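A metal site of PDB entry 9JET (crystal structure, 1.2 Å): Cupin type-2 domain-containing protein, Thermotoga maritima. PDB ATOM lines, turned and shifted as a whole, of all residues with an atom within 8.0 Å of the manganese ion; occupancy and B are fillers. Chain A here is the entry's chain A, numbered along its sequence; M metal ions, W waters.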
ATOM      1  N   LYS A  22     -31.730  24.315  13.810  1.00  0.00           N
ATOM      2  CA  LYS A  22     -30.373  24.790  14.075  1.00  0.00           C
ATOM      3  C   LYS A  22     -30.102  26.142  13.416  1.00  0.00           C
ATOM      4  O   LYS A  22     -28.961  26.591  13.462  1.00  0.00           O
ATOM      5  CB  LYS A  22     -29.371  23.743  13.621  1.00  0.00           C
ATOM      6  CG  LYS A  22     -29.512  23.226  12.204  1.00  0.00           C
ATOM      7  CD  LYS A  22     -28.591  22.028  11.984  1.00  0.00           C
ATOM      8  CE  LYS A  22     -28.600  21.598  10.526  1.00  0.00           C
ATOM      9  NZ  LYS A  22     -27.599  20.532  10.291  1.00  0.00           N
ATOM     10  N   ARG A  43     -25.193  30.757  -3.384  1.00  0.00           N
ATOM     11  CA  ARG A  43     -26.220  31.347  -2.544  1.00  0.00           C
ATOM     12  C   ARG A  43     -25.695  32.604  -1.870  1.00  0.00           C
ATOM     13  O   ARG A  43     -24.497  32.729  -1.623  1.00  0.00           O
ATOM     14  CB  ARG A  43     -26.679  30.368  -1.472  1.00  0.00           C
ATOM     15  CG  ARG A  43     -27.188  29.038  -2.009  1.00  0.00           C
ATOM     16  CD  ARG A  43     -26.143  27.953  -2.052  1.00  0.00           C
ATOM     17  NE  ARG A  43     -25.503  27.597  -0.773  1.00  0.00           N
ATOM     18  CZ  ARG A  43     -25.977  26.880   0.217  1.00  0.00           C
ATOM     19  NH1 ARG A  43     -25.286  26.614   1.344  1.00  0.00           N
ATOM     20  NH2 ARG A  43     -27.188  26.373   0.159  1.00  0.00           N
ATOM     21  N   PHE A  45     -26.454  34.545   1.622  1.00  0.00           N
ATOM     22  CA  PHE A  45     -27.089  34.473   2.929  1.00  0.00           C
ATOM     23  C   PHE A  45     -27.107  35.837   3.601  1.00  0.00           C
ATOM     24  O   PHE A  45     -26.112  36.575   3.548  1.00  0.00           O
ATOM     25  CB  PHE A  45     -26.358  33.496   3.851  1.00  0.00           C
ATOM     26  CG  PHE A  45     -26.693  32.060   3.564  1.00  0.00           C
ATOM     27  CD1 PHE A  45     -27.744  31.431   4.221  1.00  0.00           C
ATOM     28  CD2 PHE A  45     -25.995  31.329   2.635  1.00  0.00           C
ATOM     29  CE1 PHE A  45     -28.056  30.121   3.927  1.00  0.00           C
ATOM     30  CE2 PHE A  45     -26.262  30.003   2.365  1.00  0.00           C
ATOM     31  CZ  PHE A  45     -27.316  29.381   3.017  1.00  0.00           C
ATOM     32  N   ILE A  53     -26.659  30.448  13.043  1.00  0.00           N
ATOM     33  CA  ILE A  53     -26.504  29.146  12.431  1.00  0.00           C
ATOM     34  C   ILE A  53     -25.685  28.302  13.379  1.00  0.00           C
ATOM     35  O   ILE A  53     -24.474  28.501  13.492  1.00  0.00           O
ATOM     36  CB  ILE A  53     -25.854  29.274  11.042  1.00  0.00           C
ATOM     37  CG1 ILE A  53     -26.701  30.135  10.121  1.00  0.00           C
ATOM     38  CG2 ILE A  53     -25.585  27.890  10.465  1.00  0.00           C
ATOM     39  CD1 ILE A  53     -25.995  30.579   8.865  1.00  0.00           C
ATOM     40  N   ASP A  54     -26.328  27.403  14.100  1.00  0.00           N
ATOM     41  CA  ASP A  54     -25.690  26.613  15.153  1.00  0.00           C
ATOM     42  C   ASP A  54     -24.572  25.769  14.531  1.00  0.00           C
ATOM     43  O   ASP A  54     -24.611  25.390  13.371  1.00  0.00           O
ATOM     44  CB  ASP A  54     -26.612  25.675  15.909  1.00  0.00           C
ATOM     45  CG  ASP A  54     -27.755  26.212  16.710  1.00  0.00           C
ATOM     46  OD1 ASP A  54     -27.684  27.424  17.058  1.00  0.00           O
ATOM     47  OD2 ASP A  54     -28.705  25.453  16.991  1.00  0.00           O
ATOM     48  N   ARG A  55     -23.607  25.448  15.382  1.00  0.00           N
ATOM     49  CA  ARG A  55     -22.559  24.509  15.000  1.00  0.00           C
ATOM     50  C   ARG A  55     -23.158  23.236  14.411  1.00  0.00           C
ATOM     51  O   ARG A  55     -24.065  22.638  14.985  1.00  0.00           O
ATOM     52  CB  ARG A  55     -21.658  24.149  16.183  1.00  0.00           C
ATOM     53  CG  ARG A  55     -20.673  25.229  16.585  1.00  0.00           C
ATOM     54  CD  ARG A  55     -19.849  24.794  17.795  1.00  0.00           C
ATOM     55  NE  ARG A  55     -18.808  25.774  18.089  1.00  0.00           N
ATOM     56  CZ  ARG A  55     -18.940  26.857  18.834  1.00  0.00           C
ATOM     57  NH1 ARG A  55     -20.110  27.130  19.406  1.00  0.00           N
ATOM     58  NH2 ARG A  55     -17.906  27.654  19.004  1.00  0.00           N
ATOM     59  N   HIS A  56     -22.594  22.815  13.285  1.00  0.00           N
ATOM     60  CA  HIS A  56     -23.042  21.650  12.550  1.00  0.00           C
ATOM     61  C   HIS A  56     -21.924  21.211  11.598  1.00  0.00           C
ATOM     62  O   HIS A  56     -20.903  21.893  11.472  1.00  0.00           O
ATOM     63  CB  HIS A  56     -24.329  21.909  11.762  1.00  0.00           C
ATOM     64  CG  HIS A  56     -24.102  22.905  10.662  1.00  0.00           C
ATOM     65  ND1 HIS A  56     -23.919  24.252  10.876  1.00  0.00           N
ATOM     66  CD2 HIS A  56     -24.014  22.720   9.333  1.00  0.00           C
ATOM     67  CE1 HIS A  56     -23.744  24.839   9.690  1.00  0.00           C
ATOM     68  NE2 HIS A  56     -23.772  23.929   8.719  1.00  0.00           N
ATOM     69  N   SER A  57     -22.132  20.081  10.954  1.00  0.00           N
ATOM     70  CA  SER A  57     -21.208  19.650   9.912  1.00  0.00           C
ATOM     71  C   SER A  57     -21.968  18.861   8.855  1.00  0.00           C
ATOM     72  O   SER A  57     -23.077  18.393   9.113  1.00  0.00           O
ATOM     73  CB  SER A  57     -20.093  18.784  10.498  1.00  0.00           C
ATOM     74  OG  SER A  57     -20.640  17.626  11.087  1.00  0.00           O
ATOM     75  N   HIS A  58     -21.349  18.743   7.692  1.00  0.00           N
ATOM     76  CA  HIS A  58     -21.966  17.972   6.615  1.00  0.00           C
ATOM     77  C   HIS A  58     -20.861  17.430   5.722  1.00  0.00           C
ATOM     78  O   HIS A  58     -19.743  17.941   5.764  1.00  0.00           O
ATOM     79  CB  HIS A  58     -22.996  18.723   5.772  1.00  0.00           C
ATOM     80  CG  HIS A  58     -22.649  20.173   5.717  1.00  0.00           C
ATOM     81  ND1 HIS A  58     -21.501  20.664   5.115  1.00  0.00           N
ATOM     82  CD2 HIS A  58     -23.288  21.241   6.223  1.00  0.00           C
ATOM     83  CE1 HIS A  58     -21.488  21.998   5.269  1.00  0.00           C
ATOM     84  NE2 HIS A  58     -22.558  22.380   5.945  1.00  0.00           N
ATOM     85  N   TRP A  60     -19.839  17.752   2.778  1.00  0.00           N
ATOM     86  CA  TRP A  60     -19.362  18.576   1.700  1.00  0.00           C
ATOM     87  C   TRP A  60     -18.751  19.838   2.304  1.00  0.00           C
ATOM     88  O   TRP A  60     -19.039  20.222   3.436  1.00  0.00           O
ATOM     89  CB  TRP A  60     -20.467  18.977   0.722  1.00  0.00           C
ATOM     90  CG  TRP A  60     -21.649  19.646   1.336  1.00  0.00           C
ATOM     91  CD1 TRP A  60     -21.831  20.968   1.620  1.00  0.00           C
ATOM     92  CD2 TRP A  60     -22.867  18.997   1.753  1.00  0.00           C
ATOM     93  NE1 TRP A  60     -23.053  21.180   2.184  1.00  0.00           N
ATOM     94  CE2 TRP A  60     -23.713  19.995   2.272  1.00  0.00           C
ATOM     95  CE3 TRP A  60     -23.300  17.672   1.722  1.00  0.00           C
ATOM     96  CZ2 TRP A  60     -24.976  19.686   2.762  1.00  0.00           C
ATOM     97  CZ3 TRP A  60     -24.561  17.377   2.214  1.00  0.00           C
ATOM     98  CH2 TRP A  60     -25.386  18.379   2.726  1.00  0.00           C
ATOM     99  N   GLU A  61     -17.892  20.465   1.516  1.00  0.00           N
ATOM    100  CA  GLU A  61     -17.211  21.695   1.850  1.00  0.00           C
ATOM    101  C   GLU A  61     -18.093  22.931   1.646  1.00  0.00           C
ATOM    102  O   GLU A  61     -19.093  22.862   0.943  1.00  0.00           O
ATOM    103  CB  GLU A  61     -15.963  21.860   0.974  1.00  0.00           C
ATOM    104  CG  GLU A  61     -16.210  22.133  -0.499  1.00  0.00           C
ATOM    105  CD  GLU A  61     -16.495  20.960  -1.397  1.00  0.00           C
ATOM    106  OE1 GLU A  61     -16.848  19.882  -0.884  1.00  0.00           O
ATOM    107  OE2 GLU A  61     -16.385  21.138  -2.638  1.00  0.00           O
ATOM    108  N   HIS A  62     -17.674  24.017   2.264  1.00  0.00           N
ATOM    109  CA  HIS A  62     -18.210  25.348   1.975  1.00  0.00           C
ATOM    110  C   HIS A  62     -17.076  26.265   1.488  1.00  0.00           C
ATOM    111  O   HIS A  62     -15.998  26.210   2.050  1.00  0.00           O
ATOM    112  CB  HIS A  62     -18.825  26.063   3.159  1.00  0.00           C
ATOM    113  CG  HIS A  62     -20.112  25.727   3.764  1.00  0.00           C
ATOM    114  ND1 HIS A  62     -21.321  25.807   3.121  1.00  0.00           N
ATOM    115  CD2 HIS A  62     -20.415  25.378   5.048  1.00  0.00           C
ATOM    116  CE1 HIS A  62     -22.293  25.472   3.942  1.00  0.00           C
ATOM    117  NE2 HIS A  62     -21.773  25.189   5.132  1.00  0.00           N
ATOM    118  N   ILE A  64     -16.862  30.414   1.163  1.00  0.00           N
ATOM    119  CA  ILE A  64     -17.621  31.594   1.561  1.00  0.00           C
ATOM    120  C   ILE A  64     -16.833  32.866   1.287  1.00  0.00           C
ATOM    121  O   ILE A  64     -15.617  32.886   1.446  1.00  0.00           O
ATOM    122  CB  ILE A  64     -17.959  31.470   3.069  1.00  0.00           C
ATOM    123  CG1 ILE A  64     -19.002  30.358   3.285  1.00  0.00           C
ATOM    124  CG2 ILE A  64     -18.373  32.782   3.700  1.00  0.00           C
ATOM    125  CD1 ILE A  64     -19.166  29.885   4.703  1.00  0.00           C
ATOM    126  N   VAL A  90     -14.339  25.914   4.489  1.00  0.00           N
ATOM    127  CA  VAL A  90     -14.724  24.928   5.479  1.00  0.00           C
ATOM    128  C   VAL A  90     -14.581  23.535   4.865  1.00  0.00           C
ATOM    129  O   VAL A  90     -15.252  23.235   3.882  1.00  0.00           O
ATOM    130  CB  VAL A  90     -16.152  25.123   6.005  1.00  0.00           C
ATOM    131  CG1 VAL A  90     -16.400  24.196   7.195  1.00  0.00           C
ATOM    132  CG2 VAL A  90     -16.437  26.558   6.447  1.00  0.00           C
ATOM    133  N   GLU A  94     -16.086  19.413   8.748  1.00  0.00           N
ATOM    134  CA  GLU A  94     -15.596  20.303   9.800  1.00  0.00           C
ATOM    135  C   GLU A  94     -16.743  20.986  10.501  1.00  0.00           C
ATOM    136  O   GLU A  94     -17.696  21.481   9.859  1.00  0.00           O
ATOM    137  CB  GLU A  94     -14.660  21.335   9.159  1.00  0.00           C
ATOM    138  CG  GLU A  94     -13.947  22.305  10.075  1.00  0.00           C
ATOM    139  CD  GLU A  94     -12.836  23.102   9.437  1.00  0.00           C
ATOM    140  OE1 GLU A  94     -12.746  23.319   8.213  1.00  0.00           O
ATOM    141  OE2 GLU A  94     -11.972  23.557  10.224  1.00  0.00           O
ATOM    142  N   ILE A  95     -16.717  21.020  11.830  1.00  0.00           N
ATOM    143  CA  ILE A  95     -17.737  21.689  12.589  1.00  0.00           C
ATOM    144  C   ILE A  95     -17.621  23.203  12.377  1.00  0.00           C
ATOM    145  O   ILE A  95     -16.545  23.806  12.373  1.00  0.00           O
ATOM    146  CB  ILE A  95     -17.636  21.326  14.087  1.00  0.00           C
ATOM    147  CG1 ILE A  95     -18.030  19.859  14.353  1.00  0.00           C
ATOM    148  CG2 ILE A  95     -18.475  22.216  14.985  1.00  0.00           C
ATOM    149  CD1 ILE A  95     -17.442  19.290  15.613  1.00  0.00           C
ATOM    150  N   HIS A  96     -18.757  23.847  12.136  1.00  0.00           N
ATOM    151  CA  HIS A  96     -18.801  25.278  11.886  1.00  0.00           C
ATOM    152  C   HIS A  96     -20.202  25.809  12.153  1.00  0.00           C
ATOM    153  O   HIS A  96     -21.178  25.092  12.103  1.00  0.00           O
ATOM    154  CB  HIS A  96     -18.402  25.574  10.427  1.00  0.00           C
ATOM    155  CG  HIS A  96     -19.362  25.011   9.432  1.00  0.00           C
ATOM    156  ND1 HIS A  96     -19.376  23.650   9.187  1.00  0.00           N
ATOM    157  CD2 HIS A  96     -20.322  25.529   8.624  1.00  0.00           C
ATOM    158  CE1 HIS A  96     -20.307  23.392   8.279  1.00  0.00           C
ATOM    159  NE2 HIS A  96     -20.917  24.505   7.915  1.00  0.00           N
ATOM    160  N   GLY A  97     -20.284  27.106  12.433  1.00  0.00           N
ATOM    161  CA  GLY A  97     -21.542  27.808  12.521  1.00  0.00           C
ATOM    162  C   GLY A  97     -21.271  29.297  12.418  1.00  0.00           C
ATOM    163  O   GLY A  97     -20.128  29.695  12.225  1.00  0.00           O
ATOM    164  N   PHE A  98     -22.320  30.109  12.537  1.00  0.00           N
ATOM    165  CA  PHE A  98     -22.191  31.546  12.350  1.00  0.00           C
ATOM    166  C   PHE A  98     -23.128  32.315  13.272  1.00  0.00           C
ATOM    167  O   PHE A  98     -24.221  31.806  13.554  1.00  0.00           O
ATOM    168  CB  PHE A  98     -22.508  31.952  10.902  1.00  0.00           C
ATOM    169  CG  PHE A  98     -21.654  31.197   9.913  1.00  0.00           C
ATOM    170  CD1 PHE A  98     -20.343  31.584   9.654  1.00  0.00           C
ATOM    171  CD2 PHE A  98     -22.185  30.066   9.293  1.00  0.00           C
ATOM    172  CE1 PHE A  98     -19.571  30.841   8.782  1.00  0.00           C
ATOM    173  CE2 PHE A  98     -21.406  29.344   8.411  1.00  0.00           C
ATOM    174  CZ  PHE A  98     -20.111  29.733   8.165  1.00  0.00           C
ATOM    175  N   CSD A 110     -22.110  31.929  -0.308  1.00  0.00           N
ATOM    176  CA  CSD A 110     -21.779  30.561   0.178  1.00  0.00           C
ATOM    177  CB  CSD A 110     -22.658  30.230   1.325  1.00  0.00           C
ATOM    178  SG  CSD A 110     -22.248  28.674   2.129  1.00  0.00           S
ATOM    179  C   CSD A 110     -22.030  29.618  -1.019  1.00  0.00           C
ATOM    180  O   CSD A 110     -23.136  29.590  -1.558  1.00  0.00           O
ATOM    181  OD1 CSD A 110     -23.222  28.602   3.240  1.00  0.00           O
ATOM    182  OD2 CSD A 110     -22.654  27.738   1.090  1.00  0.00           O
ATOM    183  N   ILE A 112     -21.439  25.594  -2.445  1.00  0.00           N
ATOM    184  CA  ILE A 112     -21.286  24.201  -2.117  1.00  0.00           C
ATOM    185  C   ILE A 112     -21.372  23.358  -3.397  1.00  0.00           C
ATOM    186  O   ILE A 112     -22.026  23.784  -4.376  1.00  0.00           O
ATOM    187  CB  ILE A 112     -22.354  23.716  -1.112  1.00  0.00           C
ATOM    188  CG1 ILE A 112     -23.782  23.831  -1.614  1.00  0.00           C
ATOM    189  CG2 ILE A 112     -22.161  24.434   0.217  1.00  0.00           C
ATOM    190  CD1 ILE A 112     -24.820  23.211  -0.695  1.00  0.00           C
HETATM  191 MN    MN M   1     -22.757  24.390   6.802  1.00  0.00          MN
HETATM  192  O   HOH W   1     -24.819  24.336   5.793  1.00  0.00           O
HETATM  193  O   HOH W   2     -23.504  26.515   7.187  1.00  0.00           O
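A ring nitrogen (ND1) of His 96 is in hydrogen-bond range of the backbone carbonyl oxygen (O) of Glu 94 (2.8 Å). ND1 of His 58 sits at hydrogen-bond distance from O of Trp 60 (3.0 Å). OD2 of CSD 110 sits at hydrogen-bond distance from a ring nitrogen (ND1) of His 62, 3.1 Å away. ND1 of His 56 lies within hydrogen-bond range of O of Asp 54. O of His 62 sits at hydrogen-bond distance from N of Val 90, 3.0 Å away.
The manganese ion is bound by NE2 of His 62 (2.1 Å), NE2 of His 96 (2.2 Å), NE2 of His 58 (2.2 Å), NE2 of His 56 (2.2 Å), water W2 (2.3 Å) and water W1 (2.3 Å).
Four residues have an atom within 4 Å of the manganese ion: His 56, His 58, His 62 and His 96. The nearest printed residue that does not touch the manganese ion is Phe 98 (5.4 Å).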
